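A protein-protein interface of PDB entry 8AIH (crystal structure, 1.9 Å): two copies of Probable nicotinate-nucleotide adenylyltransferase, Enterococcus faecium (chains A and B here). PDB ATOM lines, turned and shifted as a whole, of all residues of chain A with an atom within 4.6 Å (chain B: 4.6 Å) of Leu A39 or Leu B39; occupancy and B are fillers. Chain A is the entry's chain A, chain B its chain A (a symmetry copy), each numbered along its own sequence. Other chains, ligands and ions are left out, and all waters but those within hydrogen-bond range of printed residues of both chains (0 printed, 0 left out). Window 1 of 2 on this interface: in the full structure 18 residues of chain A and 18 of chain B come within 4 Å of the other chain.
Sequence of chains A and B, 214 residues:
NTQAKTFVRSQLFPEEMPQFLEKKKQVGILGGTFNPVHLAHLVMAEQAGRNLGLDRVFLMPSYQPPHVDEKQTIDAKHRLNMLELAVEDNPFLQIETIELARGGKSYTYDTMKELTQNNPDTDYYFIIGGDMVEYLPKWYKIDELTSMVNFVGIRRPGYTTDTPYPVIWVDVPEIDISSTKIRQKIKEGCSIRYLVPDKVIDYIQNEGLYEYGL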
ATOM      1  N   HIS A  38      12.883 -14.490  16.435  1.00  0.00           N
ATOM      2  CA  HIS A  38      14.291 -14.522  16.805  1.00  0.00           C
ATOM      3  C   HIS A  38      14.565 -15.908  17.349  1.00  0.00           C
ATOM      4  O   HIS A  38      13.636 -16.701  17.521  1.00  0.00           O
ATOM      5  CB  HIS A  38      14.647 -13.446  17.832  1.00  0.00           C
ATOM      6  CG  HIS A  38      13.685 -13.386  18.958  1.00  0.00           C
ATOM      7  ND1 HIS A  38      13.475 -14.458  19.794  1.00  0.00           N
ATOM      8  CD2 HIS A  38      12.888 -12.391  19.409  1.00  0.00           C
ATOM      9  CE1 HIS A  38      12.591 -14.125  20.717  1.00  0.00           C
ATOM     10  NE2 HIS A  38      12.220 -12.875  20.507  1.00  0.00           N
ATOM     11  N   LEU A  39      15.843 -16.226  17.566  1.00  0.00           N
ATOM     12  CA  LEU A  39      16.204 -17.612  17.849  1.00  0.00           C
ATOM     13  C   LEU A  39      15.549 -18.139  19.121  1.00  0.00           C
ATOM     14  O   LEU A  39      15.425 -19.360  19.288  1.00  0.00           O
ATOM     15  CB  LEU A  39      17.723 -17.793  17.968  1.00  0.00           C
ATOM     16  CG  LEU A  39      17.948 -19.185  17.326  1.00  0.00           C
ATOM     17  CD1 LEU A  39      17.912 -19.088  15.782  1.00  0.00           C
ATOM     18  CD2 LEU A  39      19.101 -19.956  17.807  1.00  0.00           C
ATOM     19  N   ALA A  40      15.117 -17.258  20.020  1.00  0.00           N
ATOM     20  CA  ALA A  40      14.469 -17.743  21.243  1.00  0.00           C
ATOM     21  C   ALA A  40      13.125 -18.416  20.924  1.00  0.00           C
ATOM     22  O   ALA A  40      12.797 -19.467  21.503  1.00  0.00           O
ATOM     23  CB  ALA A  40      14.291 -16.591  22.231  1.00  0.00           C
ATOM     24  N   HIS A  41      12.381 -17.877  19.938  1.00  0.00           N
ATOM     25  CA  HIS A  41      11.120 -18.495  19.498  1.00  0.00           C
ATOM     26  C   HIS A  41      11.330 -19.892  18.920  1.00  0.00           C
ATOM     27  O   HIS A  41      10.551 -20.820  19.203  1.00  0.00           O
ATOM     28  CB  HIS A  41      10.422 -17.607  18.458  1.00  0.00           C
ATOM     29  CG  HIS A  41      10.041 -16.263  18.987  1.00  0.00           C
ATOM     30  ND1 HIS A  41      10.289 -15.091  18.304  1.00  0.00           N
ATOM     31  CD2 HIS A  41       9.399 -15.902  20.135  1.00  0.00           C
ATOM     32  CE1 HIS A  41       9.849 -14.060  19.013  1.00  0.00           C
ATOM     33  NE2 HIS A  41       9.299 -14.527  20.123  1.00  0.00           N
ATOM     34  N   LEU A  42      12.364 -20.059  18.103  1.00  0.00           N
ATOM     35  CA  LEU A  42      12.601 -21.337  17.419  1.00  0.00           C
ATOM     36  C   LEU A  42      13.052 -22.431  18.394  1.00  0.00           C
ATOM     37  O   LEU A  42      12.558 -23.579  18.358  1.00  0.00           O
ATOM     38  CB  LEU A  42      13.653 -21.129  16.340  1.00  0.00           C
ATOM     39  CG  LEU A  42      13.197 -20.175  15.240  1.00  0.00           C
ATOM     40  CD1 LEU A  42      14.382 -19.753  14.373  1.00  0.00           C
ATOM     41  CD2 LEU A  42      12.095 -20.852  14.374  1.00  0.00           C
ATOM     42  N   VAL A  43      14.051 -22.116  19.208  1.00  0.00           N
ATOM     43  CA  VAL A  43      14.492 -23.014  20.276  1.00  0.00           C
ATOM     44  C   VAL A  43      13.310 -23.393  21.172  1.00  0.00           C
ATOM     45  O   VAL A  43      13.086 -24.575  21.454  1.00  0.00           O
ATOM     46  CB  VAL A  43      15.620 -22.355  21.095  1.00  0.00           C
ATOM     47  CG1 VAL A  43      15.863 -23.154  22.435  1.00  0.00           C
ATOM     48  CG2 VAL A  43      16.882 -22.213  20.261  1.00  0.00           C
ATOM     49  N   ILE A 175      16.963 -18.863  26.788  1.00  0.00           N
ATOM     50  CA  ILE A 175      17.533 -18.016  25.748  1.00  0.00           C
ATOM     51  C   ILE A 175      16.966 -16.628  26.015  1.00  0.00           C
ATOM     52  O   ILE A 175      15.791 -16.372  25.748  1.00  0.00           O
ATOM     53  CB  ILE A 175      17.179 -18.530  24.349  1.00  0.00           C
ATOM     54  CG1 ILE A 175      17.760 -19.921  24.148  1.00  0.00           C
ATOM     55  CG2 ILE A 175      17.746 -17.628  23.259  1.00  0.00           C
ATOM     56  CD1 ILE A 175      18.066 -20.190  22.682  1.00  0.00           C
ATOM     57  N   ILE A 177      16.504 -13.697  24.905  1.00  0.00           N
ATOM     58  CA  ILE A 177      16.324 -12.837  23.750  1.00  0.00           C
ATOM     59  C   ILE A 177      14.858 -12.425  23.772  1.00  0.00           C
ATOM     60  O   ILE A 177      13.982 -13.281  23.943  1.00  0.00           O
ATOM     61  CB  ILE A 177      16.684 -13.603  22.459  1.00  0.00           C
ATOM     62  CG1 ILE A 177      18.172 -13.969  22.442  1.00  0.00           C
ATOM     63  CG2 ILE A 177      16.381 -12.780  21.221  1.00  0.00           C
ATOM     64  CD1 ILE A 177      18.562 -14.839  21.255  1.00  0.00           C
ATOM     65  N   TYR A 194      23.139 -14.169  14.755  1.00  0.00           N
ATOM     66  CA  TYR A 194      22.971 -15.387  15.554  1.00  0.00           C
ATOM     67  C   TYR A 194      21.775 -15.280  16.507  1.00  0.00           C
ATOM     68  O   TYR A 194      21.142 -16.295  16.822  1.00  0.00           O
ATOM     69  CB  TYR A 194      24.272 -15.740  16.304  1.00  0.00           C
ATOM     70  CG  TYR A 194      25.550 -15.960  15.458  1.00  0.00           C
ATOM     71  CD1 TYR A 194      25.629 -16.984  14.518  1.00  0.00           C
ATOM     72  CD2 TYR A 194      26.653 -15.132  15.583  1.00  0.00           C
ATOM     73  CE1 TYR A 194      26.792 -17.195  13.763  1.00  0.00           C
ATOM     74  CE2 TYR A 194      27.813 -15.334  14.824  1.00  0.00           C
ATOM     75  CZ  TYR A 194      27.874 -16.356  13.907  1.00  0.00           C
ATOM     76  OH  TYR A 194      29.020 -16.550  13.149  1.00  0.00           O
ATOM     77  N   LEU A 195      21.421 -14.047  16.912  1.00  0.00           N
ATOM     78  CA  LEU A 195      20.214 -13.774  17.700  1.00  0.00           C
ATOM     79  C   LEU A 195      18.951 -13.946  16.871  1.00  0.00           C
ATOM     80  O   LEU A 195      17.892 -14.330  17.405  1.00  0.00           O
ATOM     81  CB  LEU A 195      20.259 -12.333  18.248  1.00  0.00           C
ATOM     82  CG  LEU A 195      21.441 -11.922  19.155  1.00  0.00           C
ATOM     83  CD1 LEU A 195      21.420 -10.431  19.527  1.00  0.00           C
ATOM     84  CD2 LEU A 195      21.631 -12.833  20.399  1.00  0.00           C
ATOM     85  N   VAL A 196      19.057 -13.654  15.567  1.00  0.00           N
ATOM     86  CA  VAL A 196      17.973 -13.587  14.598  1.00  0.00           C
ATOM     87  C   VAL A 196      18.468 -14.321  13.354  1.00  0.00           C
ATOM     88  O   VAL A 196      19.647 -14.185  12.967  1.00  0.00           O
ATOM     89  CB  VAL A 196      17.567 -12.137  14.273  1.00  0.00           C
ATOM     90  CG1 VAL A 196      16.332 -12.136  13.476  1.00  0.00           C
ATOM     91  CG2 VAL A 196      17.301 -11.346  15.610  1.00  0.00           C
ATOM     92  N   PRO A 197      17.633 -15.175  12.766  1.00  0.00           N
ATOM     93  CA  PRO A 197      18.073 -15.996  11.621  1.00  0.00           C
ATOM     94  C   PRO A 197      18.615 -15.160  10.471  1.00  0.00           C
ATOM     95  O   PRO A 197      18.152 -14.039  10.227  1.00  0.00           O
ATOM     96  CB  PRO A 197      16.792 -16.733  11.214  1.00  0.00           C
ATOM     97  CG  PRO A 197      15.956 -16.794  12.520  1.00  0.00           C
ATOM     98  CD  PRO A 197      16.278 -15.514  13.232  1.00  0.00           C
ATOM     99  N   HIS B  38      28.558 -24.645  19.662  1.00  0.00           N
ATOM    100  CA  HIS B  38      27.107 -24.544  19.720  1.00  0.00           C
ATOM    101  C   HIS B  38      26.775 -23.068  19.742  1.00  0.00           C
ATOM    102  O   HIS B  38      27.676 -22.231  19.839  1.00  0.00           O
ATOM    103  CB  HIS B  38      26.522 -25.259  20.939  1.00  0.00           C
ATOM    104  CG  HIS B  38      27.242 -24.936  22.194  1.00  0.00           C
ATOM    105  ND1 HIS B  38      27.317 -23.651  22.680  1.00  0.00           N
ATOM    106  CD2 HIS B  38      27.902 -25.716  23.079  1.00  0.00           C
ATOM    107  CE1 HIS B  38      27.992 -23.653  23.816  1.00  0.00           C
ATOM    108  NE2 HIS B  38      28.357 -24.894  24.081  1.00  0.00           N
ATOM    109  N   LEU B  39      25.489 -22.739  19.594  1.00  0.00           N
ATOM    110  CA  LEU B  39      25.124 -21.345  19.356  1.00  0.00           C
ATOM    111  C   LEU B  39      25.533 -20.429  20.504  1.00  0.00           C
ATOM    112  O   LEU B  39      25.660 -19.213  20.306  1.00  0.00           O
ATOM    113  CB  LEU B  39      23.617 -21.184  19.113  1.00  0.00           C
ATOM    114  CG  LEU B  39      23.567 -20.068  18.040  1.00  0.00           C
ATOM    115  CD1 LEU B  39      23.902 -20.638  16.640  1.00  0.00           C
ATOM    116  CD2 LEU B  39      22.367 -19.222  18.021  1.00  0.00           C
ATOM    117  N   ALA B  40      25.751 -20.973  21.699  1.00  0.00           N
ATOM    118  CA  ALA B  40      26.162 -20.112  22.813  1.00  0.00           C
ATOM    119  C   ALA B  40      27.563 -19.529  22.572  1.00  0.00           C
ATOM    120  O   ALA B  40      27.804 -18.341  22.848  1.00  0.00           O
ATOM    121  CB  ALA B  40      26.106 -20.894  24.125  1.00  0.00           C
ATOM    122  N   HIS B  41      28.469 -20.324  21.968  1.00  0.00           N
ATOM    123  CA  HIS B  41      29.811 -19.833  21.614  1.00  0.00           C
ATOM    124  C   HIS B  41      29.762 -18.693  20.602  1.00  0.00           C
ATOM    125  O   HIS B  41      30.500 -17.698  20.730  1.00  0.00           O
ATOM    126  CB  HIS B  41      30.671 -20.979  21.059  1.00  0.00           C
ATOM    127  CG  HIS B  41      30.898 -22.079  22.043  1.00  0.00           C
ATOM    128  ND1 HIS B  41      30.752 -23.412  21.724  1.00  0.00           N
ATOM    129  CD2 HIS B  41      31.291 -22.046  23.349  1.00  0.00           C
ATOM    130  CE1 HIS B  41      31.011 -24.158  22.789  1.00  0.00           C
ATOM    131  NE2 HIS B  41      31.347 -23.352  23.785  1.00  0.00           N
ATOM    132  N   LEU B  42      28.915 -18.820  19.587  1.00  0.00           N
ATOM    133  CA  LEU B  42      28.857 -17.825  18.508  1.00  0.00           C
ATOM    134  C   LEU B  42      28.258 -16.498  18.987  1.00  0.00           C
ATOM    135  O   LEU B  42      28.786 -15.403  18.694  1.00  0.00           O
ATOM    136  CB  LEU B  42      28.031 -18.392  17.362  1.00  0.00           C
ATOM    137  CG  LEU B  42      28.664 -19.624  16.725  1.00  0.00           C
ATOM    138  CD1 LEU B  42      27.660 -20.332  15.817  1.00  0.00           C
ATOM    139  CD2 LEU B  42      29.936 -19.215  15.925  1.00  0.00           C
ATOM    140  N   VAL B  43      27.109 -16.576  19.645  1.00  0.00           N
ATOM    141  CA  VAL B  43      26.496 -15.405  20.273  1.00  0.00           C
ATOM    142  C   VAL B  43      27.490 -14.730  21.221  1.00  0.00           C
ATOM    143  O   VAL B  43      27.692 -13.512  21.160  1.00  0.00           O
ATOM    144  CB  VAL B  43      25.209 -15.813  21.018  1.00  0.00           C
ATOM    145  CG1 VAL B  43      24.733 -14.645  21.969  1.00  0.00           C
ATOM    146  CG2 VAL B  43      24.131 -16.247  20.039  1.00  0.00           C
ATOM    147  N   ILE B 175      22.665 -17.406  27.134  1.00  0.00           N
ATOM    148  CA  ILE B 175      22.284 -18.551  26.318  1.00  0.00           C
ATOM    149  C   ILE B 175      22.743 -19.770  27.108  1.00  0.00           C
ATOM    150  O   ILE B 175      23.939 -20.058  27.169  1.00  0.00           O
ATOM    151  CB  ILE B 175      22.922 -18.486  24.926  1.00  0.00           C
ATOM    152  CG1 ILE B 175      22.435 -17.245  24.193  1.00  0.00           C
ATOM    153  CG2 ILE B 175      22.551 -19.700  24.080  1.00  0.00           C
ATOM    154  CD1 ILE B 175      22.431 -17.454  22.686  1.00  0.00           C
ATOM    155  N   ILE B 177      23.321 -22.884  27.076  1.00  0.00           N
ATOM    156  CA  ILE B 177      23.697 -24.053  26.304  1.00  0.00           C
ATOM    157  C   ILE B 177      25.116 -24.392  26.740  1.00  0.00           C
ATOM    158  O   ILE B 177      25.968 -23.498  26.805  1.00  0.00           O
ATOM    159  CB  ILE B 177      23.622 -23.738  24.794  1.00  0.00           C
ATOM    160  CG1 ILE B 177      22.178 -23.443  24.373  1.00  0.00           C
ATOM    161  CG2 ILE B 177      24.136 -24.895  23.958  1.00  0.00           C
ATOM    162  CD1 ILE B 177      22.057 -22.997  22.922  1.00  0.00           C
ATOM    163  N   TYR B 194      18.826 -25.795  16.186  1.00  0.00           N
ATOM    164  CA  TYR B 194      18.872 -24.384  16.584  1.00  0.00           C
ATOM    165  C   TYR B 194      19.854 -24.153  17.739  1.00  0.00           C
ATOM    166  O   TYR B 194      20.445 -23.071  17.840  1.00  0.00           O
ATOM    167  CB  TYR B 194      17.461 -23.858  16.916  1.00  0.00           C
ATOM    168  CG  TYR B 194      16.382 -23.952  15.811  1.00  0.00           C
ATOM    169  CD1 TYR B 194      16.521 -23.272  14.603  1.00  0.00           C
ATOM    170  CD2 TYR B 194      15.250 -24.734  15.967  1.00  0.00           C
ATOM    171  CE1 TYR B 194      15.537 -23.344  13.607  1.00  0.00           C
ATOM    172  CE2 TYR B 194      14.269 -24.814  14.971  1.00  0.00           C
ATOM    173  CZ  TYR B 194      14.421 -24.130  13.789  1.00  0.00           C
ATOM    174  OH  TYR B 194      13.453 -24.217  12.799  1.00  0.00           O
ATOM    175  N   LEU B 195      20.082 -25.188  18.567  1.00  0.00           N
ATOM    176  CA  LEU B 195      21.102 -25.164  19.622  1.00  0.00           C
ATOM    177  C   LEU B 195      22.509 -25.218  19.045  1.00  0.00           C
ATOM    178  O   LEU B 195      23.453 -24.654  19.631  1.00  0.00           O
ATOM    179  CB  LEU B 195      20.905 -26.365  20.570  1.00  0.00           C
ATOM    180  CG  LEU B 195      19.555 -26.510  21.309  1.00  0.00           C
ATOM    181  CD1 LEU B 195      19.456 -27.811  22.122  1.00  0.00           C
ATOM    182  CD2 LEU B 195      19.154 -25.266  22.146  1.00  0.00           C
ATOM    183  N   VAL B 196      22.651 -25.903  17.902  1.00  0.00           N
ATOM    184  CA  VAL B 196      23.901 -26.234  17.235  1.00  0.00           C
ATOM    185  C   VAL B 196      23.684 -25.938  15.752  1.00  0.00           C
ATOM    186  O   VAL B 196      22.600 -26.224  15.203  1.00  0.00           O
ATOM    187  CB  VAL B 196      24.318 -27.700  17.462  1.00  0.00           C
ATOM    188  CG1 VAL B 196      25.685 -27.908  16.964  1.00  0.00           C
ATOM    189  CG2 VAL B 196      24.291 -28.027  19.003  1.00  0.00           C
ATOM    190  N   PRO B 197      24.644 -25.283  15.104  1.00  0.00           N
ATOM    191  CA  PRO B 197      24.464 -24.872  13.699  1.00  0.00           C
ATOM    192  C   PRO B 197      24.132 -26.041  12.782  1.00  0.00           C
ATOM    193  O   PRO B 197      24.598 -27.167  12.994  1.00  0.00           O
ATOM    194  CB  PRO B 197      25.822 -24.258  13.342  1.00  0.00           C
ATOM    195  CG  PRO B 197      26.387 -23.768  14.702  1.00  0.00           C
ATOM    196  CD  PRO B 197      25.891 -24.774  15.699  1.00  0.00           C
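Leu A39 touches just these residues of chain B: Leu B39 and Tyr B194. Leu B39 touches just these residues of chain A: Leu A39 and Tyr A194. Printed residues of chain B within 4 Å of Tyr A194: Leu B39 (3.4 Å), Leu B42 (3.8 Å) and Val B43 (3.8 Å). Printed residues of chain B within 4 Å of Val A43: Tyr B194 (3.8 Å) and Leu B195 (3.9 Å). Printed residues of chain A within 4 Å of Leu B42: Tyr A194 (3.8 Å). Of the printed residues of chain A, Leu B195 touches Val A43. Of the printed residues of chain B, Leu A42 touches Tyr B194 (3.8 Å). Ala A40 touches none of the printed residues of chain B. The nearest printed residue of chain A that does not touch Val B43 is Ile A177 (5.9 Å).
Leu A39 touches Leu B39. O of Tyr B194 touches CD2 of Leu A39, 3.4 Å away. Leu A42 touches Tyr B194. Val A43 touches Tyr B194 (CG2 to CB, 3.8 Å). CD2 of Leu B195 touches CG1 of Val A43 (3.9 Å). Leu B39 touches Tyr A194. CD2 of Tyr A194 touches O of Leu B42 (3.8 Å). CB of Tyr A194 touches CG2 of Val B43 (3.8 Å). CG1 of Val B43 touches CD2 of Leu A195, at 3.9 Å.
The backbone carbonyl oxygen (O) of Leu A195 is in hydrogen-bond range of the backbone NH (N) of Leu A39, at 2.8 Å. N of Leu B39 sits at hydrogen-bond distance from O of Leu B195.
Leu A39 touches its own counterpart, Leu B39. Leu A39 touches Tyr B194, and with the chains exchanged Tyr A194 touches Leu B39. Val A43 touches Tyr B194, and with the chains exchanged Tyr A194 touches Val B43. Val A43 touches Leu B195, and with the chains exchanged Leu A195 touches Val B43.
Printed residues of chain B that touch a printed residue of chain A: Leu B39, Leu B42, Val B43, Tyr B194 and Leu B195. Hydrophobic or aromatic side chains of chain B within 4 Å of the printed part of chain A: Leu B39, Leu B42, Val B43, Tyr B194 and Leu B195. Hydrophobic or aromatic side chains of chain A within 4 Å of the printed part of chain B: Leu A39, Leu A42, Val A43, Tyr A194 and Leu A195. Among the printed residues, 9 pairs touch across the chains. Among the printed residues, no Asp or Glu carboxylate lies within 4 Å of a Lys or Arg side-chain nitrogen of the other chain.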
